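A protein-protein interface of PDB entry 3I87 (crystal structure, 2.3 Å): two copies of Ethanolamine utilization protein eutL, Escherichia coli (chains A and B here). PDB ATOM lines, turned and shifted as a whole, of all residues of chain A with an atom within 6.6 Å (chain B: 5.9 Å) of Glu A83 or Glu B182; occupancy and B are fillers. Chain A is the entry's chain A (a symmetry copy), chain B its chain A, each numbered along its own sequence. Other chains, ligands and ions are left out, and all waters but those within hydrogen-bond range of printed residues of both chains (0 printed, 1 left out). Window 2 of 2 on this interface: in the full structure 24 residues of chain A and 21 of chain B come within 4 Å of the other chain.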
ATOM      1  N   THR A  12     -13.885  29.856  21.605  1.00  0.00           N
ATOM      2  CA  THR A  12     -15.171  29.173  21.446  1.00  0.00           C
ATOM      3  C   THR A  12     -15.648  28.453  22.717  1.00  0.00           C
ATOM      4  O   THR A  12     -16.850  28.418  22.990  1.00  0.00           O
ATOM      5  CB  THR A  12     -15.140  28.188  20.252  1.00  0.00           C
ATOM      6  OG1 THR A  12     -14.233  27.115  20.524  1.00  0.00           O
ATOM      7  CG2 THR A  12     -14.708  28.909  18.973  1.00  0.00           C
ATOM      8  N   ALA A  13     -14.718  27.886  23.487  1.00  0.00           N
ATOM      9  CA  ALA A  13     -15.059  27.201  24.741  1.00  0.00           C
ATOM     10  C   ALA A  13     -13.855  27.051  25.674  1.00  0.00           C
ATOM     11  O   ALA A  13     -12.707  27.026  25.224  1.00  0.00           O
ATOM     12  CB  ALA A  13     -15.667  25.838  24.451  1.00  0.00           C
ATOM     13  N   SER A  41     -10.615  26.005  23.452  1.00  0.00           N
ATOM     14  CA  SER A  41     -10.799  25.838  22.014  1.00  0.00           C
ATOM     15  C   SER A  41     -11.042  27.192  21.352  1.00  0.00           C
ATOM     16  O   SER A  41     -11.698  28.064  21.927  1.00  0.00           O
ATOM     17  CB  SER A  41     -11.949  24.868  21.711  1.00  0.00           C
ATOM     18  OG  SER A  41     -13.176  25.331  22.244  1.00  0.00           O
ATOM     19  N   ALA A  42     -10.489  27.355  20.149  1.00  0.00           N
ATOM     20  CA  ALA A  42     -10.618  28.587  19.365  1.00  0.00           C
ATOM     21  C   ALA A  42     -10.821  28.263  17.883  1.00  0.00           C
ATOM     22  O   ALA A  42     -10.709  27.106  17.471  1.00  0.00           O
ATOM     23  CB  ALA A  42      -9.388  29.456  19.554  1.00  0.00           C
ATOM     24  N   ASP A  43     -11.113  29.289  17.087  1.00  0.00           N
ATOM     25  CA  ASP A  43     -11.424  29.108  15.663  1.00  0.00           C
ATOM     26  C   ASP A  43     -10.274  29.495  14.721  1.00  0.00           C
ATOM     27  O   ASP A  43     -10.486  29.665  13.523  1.00  0.00           O
ATOM     28  CB  ASP A  43     -12.707  29.871  15.291  1.00  0.00           C
ATOM     29  CG  ASP A  43     -12.553  31.388  15.380  1.00  0.00           C
ATOM     30  OD1 ASP A  43     -11.487  31.880  15.811  1.00  0.00           O
ATOM     31  OD2 ASP A  43     -13.521  32.091  15.017  1.00  0.00           O
ATOM     32  N   ASP A  45      -5.939  28.550  13.937  1.00  0.00           N
ATOM     33  CA  ASP A  45      -4.897  27.560  14.192  1.00  0.00           C
ATOM     34  C   ASP A  45      -3.656  28.192  14.824  1.00  0.00           C
ATOM     35  O   ASP A  45      -3.390  28.001  16.009  1.00  0.00           O
ATOM     36  CB  ASP A  45      -4.521  26.825  12.898  1.00  0.00           C
ATOM     37  CG  ASP A  45      -5.649  25.944  12.369  1.00  0.00           C
ATOM     38  OD1 ASP A  45      -6.369  25.339  13.184  1.00  0.00           O
ATOM     39  OD2 ASP A  45      -5.811  25.848  11.134  1.00  0.00           O
ATOM     40  N   TYR A  49      -1.744  28.611  18.628  1.00  0.00           N
ATOM     41  CA  TYR A  49      -0.468  27.941  18.930  1.00  0.00           C
ATOM     42  C   TYR A  49       0.552  28.909  19.534  1.00  0.00           C
ATOM     43  O   TYR A  49       1.300  28.548  20.450  1.00  0.00           O
ATOM     44  CB  TYR A  49       0.166  27.301  17.682  1.00  0.00           C
ATOM     45  CG  TYR A  49      -0.664  26.271  16.928  1.00  0.00           C
ATOM     46  CD1 TYR A  49      -1.622  25.485  17.570  1.00  0.00           C
ATOM     47  CD2 TYR A  49      -0.450  26.056  15.570  1.00  0.00           C
ATOM     48  CE1 TYR A  49      -2.361  24.539  16.870  1.00  0.00           C
ATOM     49  CE2 TYR A  49      -1.179  25.114  14.862  1.00  0.00           C
ATOM     50  CZ  TYR A  49      -2.132  24.357  15.515  1.00  0.00           C
ATOM     51  OH  TYR A  49      -2.858  23.416  14.812  1.00  0.00           O
ATOM     52  N   ALA A  73       0.817  20.046  12.155  1.00  0.00           N
ATOM     53  CA  ALA A  73      -0.591  20.151  12.544  1.00  0.00           C
ATOM     54  C   ALA A  73      -1.370  20.938  11.485  1.00  0.00           C
ATOM     55  O   ALA A  73      -0.848  21.220  10.406  1.00  0.00           O
ATOM     56  CB  ALA A  73      -0.700  20.833  13.900  1.00  0.00           C
ATOM     57  N   ALA A  74      -2.620  21.278  11.792  1.00  0.00           N
ATOM     58  CA  ALA A  74      -3.421  22.134  10.924  1.00  0.00           C
ATOM     59  C   ALA A  74      -2.949  23.583  11.056  1.00  0.00           C
ATOM     60  O   ALA A  74      -2.590  24.023  12.148  1.00  0.00           O
ATOM     61  CB  ALA A  74      -4.890  22.023  11.279  1.00  0.00           C
ATOM     62  N   HIS A  75      -2.935  24.309   9.938  1.00  0.00           N
ATOM     63  CA  HIS A  75      -2.564  25.729   9.923  1.00  0.00           C
ATOM     64  C   HIS A  75      -3.589  26.529   9.128  1.00  0.00           C
ATOM     65  O   HIS A  75      -4.208  26.003   8.205  1.00  0.00           O
ATOM     66  CB  HIS A  75      -1.175  25.914   9.309  1.00  0.00           C
ATOM     67  CG  HIS A  75      -0.108  25.105   9.978  1.00  0.00           C
ATOM     68  ND1 HIS A  75       0.542  25.529  11.117  1.00  0.00           N
ATOM     69  CD2 HIS A  75       0.418  23.896   9.672  1.00  0.00           C
ATOM     70  CE1 HIS A  75       1.424  24.615  11.484  1.00  0.00           C
ATOM     71  NE2 HIS A  75       1.365  23.612  10.626  1.00  0.00           N
ATOM     72  N   GLY A  76      -3.770  27.795   9.495  1.00  0.00           N
ATOM     73  CA  GLY A  76      -4.685  28.689   8.779  1.00  0.00           C
ATOM     74  C   GLY A  76      -5.438  29.638   9.695  1.00  0.00           C
ATOM     75  O   GLY A  76      -5.397  29.486  10.918  1.00  0.00           O
ATOM     76  N   THR A  80     -12.116  28.250  11.276  1.00  0.00           N
ATOM     77  CA  THR A  80     -11.628  26.912  10.946  1.00  0.00           C
ATOM     78  C   THR A  80     -12.801  25.945  10.815  1.00  0.00           C
ATOM     79  O   THR A  80     -13.910  26.237  11.267  1.00  0.00           O
ATOM     80  CB  THR A  80     -10.655  26.384  12.023  1.00  0.00           C
ATOM     81  OG1 THR A  80     -11.268  26.481  13.318  1.00  0.00           O
ATOM     82  CG2 THR A  80      -9.354  27.182  12.012  1.00  0.00           C
ATOM     83  N   ALA A  81     -12.547  24.794  10.195  1.00  0.00           N
ATOM     84  CA  ALA A  81     -13.575  23.768   9.999  1.00  0.00           C
ATOM     85  C   ALA A  81     -14.155  23.265  11.326  1.00  0.00           C
ATOM     86  O   ALA A  81     -15.367  23.077  11.447  1.00  0.00           O
ATOM     87  CB  ALA A  81     -13.011  22.601   9.194  1.00  0.00           C
ATOM     88  N   GLY A  82     -13.288  23.053  12.314  1.00  0.00           N
ATOM     89  CA  GLY A  82     -13.712  22.589  13.636  1.00  0.00           C
ATOM     90  C   GLY A  82     -13.008  23.304  14.777  1.00  0.00           C
ATOM     91  O   GLY A  82     -12.492  24.413  14.608  1.00  0.00           O
ATOM     92  N   GLU A  83     -12.999  22.664  15.943  1.00  0.00           N
ATOM     93  CA  GLU A  83     -12.340  23.203  17.129  1.00  0.00           C
ATOM     94  C   GLU A  83     -10.830  22.986  17.070  1.00  0.00           C
ATOM     95  O   GLU A  83     -10.362  21.889  16.752  1.00  0.00           O
ATOM     96  CB  GLU A  83     -12.870  22.534  18.404  1.00  0.00           C
ATOM     97  CG  GLU A  83     -14.224  23.027  18.911  1.00  0.00           C
ATOM     98  CD  GLU A  83     -14.580  22.441  20.281  1.00  0.00           C
ATOM     99  OE1 GLU A  83     -13.772  21.657  20.827  1.00  0.00           O
ATOM    100  OE2 GLU A  83     -15.665  22.763  20.813  1.00  0.00           O
ATOM    101  N   VAL A  84     -10.079  24.038  17.378  1.00  0.00           N
ATOM    102  CA  VAL A  84      -8.658  23.920  17.659  1.00  0.00           C
ATOM    103  C   VAL A  84      -8.511  23.857  19.176  1.00  0.00           C
ATOM    104  O   VAL A  84      -8.725  24.860  19.863  1.00  0.00           O
ATOM    105  CB  VAL A  84      -7.877  25.126  17.111  1.00  0.00           C
ATOM    106  CG1 VAL A  84      -6.377  24.937  17.330  1.00  0.00           C
ATOM    107  CG2 VAL A  84      -8.192  25.326  15.634  1.00  0.00           C
ATOM    108  N   LEU A  85      -8.170  22.677  19.694  1.00  0.00           N
ATOM    109  CA  LEU A  85      -8.045  22.464  21.139  1.00  0.00           C
ATOM    110  C   LEU A  85      -6.583  22.519  21.595  1.00  0.00           C
ATOM    111  O   LEU A  85      -5.700  21.943  20.957  1.00  0.00           O
ATOM    112  CB  LEU A  85      -8.661  21.115  21.535  1.00  0.00           C
ATOM    113  CG  LEU A  85      -8.641  20.745  23.025  1.00  0.00           C
ATOM    114  CD1 LEU A  85      -9.440  21.741  23.851  1.00  0.00           C
ATOM    115  CD2 LEU A  85      -9.166  19.334  23.240  1.00  0.00           C
ATOM    116  N   PRO B 154     -17.373  16.989  20.050  1.00  0.00           N
ATOM    117  CA  PRO B 154     -16.266  17.881  19.705  1.00  0.00           C
ATOM    118  C   PRO B 154     -15.155  17.837  20.763  1.00  0.00           C
ATOM    119  O   PRO B 154     -15.453  17.702  21.947  1.00  0.00           O
ATOM    120  CB  PRO B 154     -16.927  19.261  19.643  1.00  0.00           C
ATOM    121  CG  PRO B 154     -18.353  18.976  19.336  1.00  0.00           C
ATOM    122  CD  PRO B 154     -18.662  17.703  20.067  1.00  0.00           C
ATOM    123  N   PRO B 155     -13.885  17.959  20.331  1.00  0.00           N
ATOM    124  CA  PRO B 155     -12.692  17.602  21.114  1.00  0.00           C
ATOM    125  C   PRO B 155     -12.613  18.144  22.544  1.00  0.00           C
ATOM    126  O   PRO B 155     -12.152  17.421  23.433  1.00  0.00           O
ATOM    127  CB  PRO B 155     -11.523  18.138  20.263  1.00  0.00           C
ATOM    128  CG  PRO B 155     -12.132  19.008  19.228  1.00  0.00           C
ATOM    129  CD  PRO B 155     -13.523  18.513  19.016  1.00  0.00           C
ATOM    130  N   LEU B 156     -13.041  19.384  22.778  1.00  0.00           N
ATOM    131  CA  LEU B 156     -13.030  19.931  24.141  1.00  0.00           C
ATOM    132  C   LEU B 156     -14.091  19.240  24.988  1.00  0.00           C
ATOM    133  O   LEU B 156     -13.800  18.787  26.098  1.00  0.00           O
ATOM    134  CB  LEU B 156     -13.236  21.449  24.159  1.00  0.00           C
ATOM    135  CG  LEU B 156     -12.995  22.110  25.528  1.00  0.00           C
ATOM    136  CD1 LEU B 156     -12.454  23.540  25.398  1.00  0.00           C
ATOM    137  CD2 LEU B 156     -14.254  22.093  26.379  1.00  0.00           C
ATOM    138  N   GLU B 157     -15.312  19.163  24.456  1.00  0.00           N
ATOM    139  CA  GLU B 157     -16.414  18.463  25.120  1.00  0.00           C
ATOM    140  C   GLU B 157     -16.105  16.984  25.347  1.00  0.00           C
ATOM    141  O   GLU B 157     -16.443  16.436  26.397  1.00  0.00           O
ATOM    142  CB  GLU B 157     -17.716  18.585  24.314  1.00  0.00           C
ATOM    143  CG  GLU B 157     -18.419  19.933  24.434  1.00  0.00           C
ATOM    144  CD  GLU B 157     -18.110  20.890  23.293  1.00  0.00           C
ATOM    145  OE1 GLU B 157     -16.950  20.923  22.806  1.00  0.00           O
ATOM    146  OE2 GLU B 157     -19.040  21.626  22.892  1.00  0.00           O
ATOM    147  N   PRO B 180      -6.394  15.197  16.816  1.00  0.00           N
ATOM    148  CA  PRO B 180      -5.342  15.622  15.881  1.00  0.00           C
ATOM    149  C   PRO B 180      -4.804  17.031  16.146  1.00  0.00           C
ATOM    150  O   PRO B 180      -5.582  17.957  16.374  1.00  0.00           O
ATOM    151  CB  PRO B 180      -6.045  15.573  14.521  1.00  0.00           C
ATOM    152  CG  PRO B 180      -7.095  14.547  14.676  1.00  0.00           C
ATOM    153  CD  PRO B 180      -7.543  14.598  16.107  1.00  0.00           C
ATOM    154  N   GLU B 182      -6.403  20.195  14.751  1.00  0.00           N
ATOM    155  CA  GLU B 182      -7.730  20.661  14.361  1.00  0.00           C
ATOM    156  C   GLU B 182      -8.606  19.501  13.910  1.00  0.00           C
ATOM    157  O   GLU B 182      -8.334  18.866  12.889  1.00  0.00           O
ATOM    158  CB  GLU B 182      -7.629  21.686  13.226  1.00  0.00           C
ATOM    159  CG  GLU B 182      -8.959  22.340  12.841  1.00  0.00           C
ATOM    160  CD  GLU B 182      -8.942  22.929  11.438  1.00  0.00           C
ATOM    161  OE1 GLU B 182      -7.922  23.544  11.055  1.00  0.00           O
ATOM    162  OE2 GLU B 182      -9.954  22.773  10.718  1.00  0.00           O
ATOM    163  N   THR B 183      -9.654  19.230  14.680  1.00  0.00           N
ATOM    164  CA  THR B 183     -10.682  18.272  14.285  1.00  0.00           C
ATOM    165  C   THR B 183     -12.037  18.765  14.779  1.00  0.00           C
ATOM    166  O   THR B 183     -12.105  19.624  15.664  1.00  0.00           O
ATOM    167  CB  THR B 183     -10.397  16.857  14.843  1.00  0.00           C
ATOM    168  OG1 THR B 183     -11.196  15.895  14.144  1.00  0.00           O
ATOM    169  CG2 THR B 183     -10.691  16.779  16.343  1.00  0.00           C
ATOM    170  N   ASN B 184     -13.109  18.231  14.201  1.00  0.00           N
ATOM    171  CA  ASN B 184     -14.462  18.614  14.611  1.00  0.00           C
ATOM    172  C   ASN B 184     -15.089  17.634  15.604  1.00  0.00           C
ATOM    173  O   ASN B 184     -15.875  18.052  16.453  1.00  0.00           O
ATOM    174  CB  ASN B 184     -15.388  18.862  13.403  1.00  0.00           C
ATOM    175  CG  ASN B 184     -15.212  17.842  12.287  1.00  0.00           C
ATOM    176  OD1 ASN B 184     -15.173  16.633  12.523  1.00  0.00           O
ATOM    177  ND2 ASN B 184     -15.118  18.333  11.057  1.00  0.00           N
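N of Leu B156 lies within hydrogen-bond range of OE1 of Glu A83, at 3.1 Å.
OE2 of Glu B182 sits at hydrogen-bond distance from N of Ala A81 (3.3 Å).
The backbone carbonyl oxygen of Thr B183 sits at hydrogen-bond distance from the backbone NH of Glu A83, 3.2 Å away.
OD2 of Asp A45 sits close to OE1 of Glu B182.
OE2 of Glu A83 sits close to OE1 of Glu B157.
O of Ala A74 is in hydrogen-bond range of OH of Tyr A49 (2.7 Å).
N of Asp A45 lies within hydrogen-bond range of O of Gly A76.
OG1 of Thr A80 sits at hydrogen-bond distance from O of Gly A82 (2.7 Å).
OD2 of Asp A45 lies close to N of His A75 (3.5 Å).
N of Thr A80 lies within hydrogen-bond range of O of Asp A43 (3.1 Å).
The side-chain hydroxyl (OG) of Ser A41 is in hydrogen-bond range of the side-chain hydroxyl (OG1) of Thr A12 (2.7 Å).
Leu B156 touches Ala A13.
Ser A41 touches Leu B156.
CB of Glu B182 touches CB of Ala A74, 3.4 Å away.
Glu B182 touches Thr A80.
N of Gly A82 touches OE2 of Glu B182, 3.7 Å away.
Glu A83 touches Pro B154.
OE1 of Glu A83 touches CG of Pro B155, 3.5 Å away.
Glu B182 touches Glu A83.
Leu A85 touches Pro B155.
CD1 of Leu A85 touches CB of Leu B156, 3.8 Å away.
Printed residues of chain B within 4 Å of Ala A74: Glu B182 (3.4 Å).
Val A84 touches none of the printed residues of chain B.
Printed residues of chain A within 4 Å of Pro B154: Glu A83 (3.9 Å).
Printed residues of chain A within 4 Å of Pro B155: Glu A83 and Leu A85.
Pro B180 touches none of the printed residues of chain A.
Glu B182 touches just these residues of chain A: Asp A45, Ala A74, Thr A80, Ala A81, Gly A82 and Glu A83.
The nearest residue of chain B that does not touch Glu A83 is Asn B184 (4.5 Å).
The nearest residue of chain A that does not touch Glu B182 is Val A84 (4.2 Å).
Of the 17 printed residues of chain A, 9 touch a printed residue of chain B.
Hydrophobic or aromatic side chains of chain A that line the printed part of chain B: Ala A74, Ala A81 and Leu A85.
Of the 8 printed residues of chain B, 6 touch a printed residue of chain A.
Printed residues of chain B that touch a printed residue of chain A: Pro B154, Pro B155, Leu B156, Glu B157, Glu B182 and Thr B183.
Hydrophobic or aromatic side chains of chain B within 4 Å of the printed part of chain A: Pro B154, Pro B155 and Leu B156.
Among the printed residues, 16 pairs touch across the chains.
Among the printed residues, no Asp or Glu carboxylate lies within 4 Å of a Lys or Arg side-chain nitrogen of the other chain.
No position is printed for both chains.
Of the 16 pairs that touch across the chains among the printed residues, none has its exchanged pair printed and touching as well.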
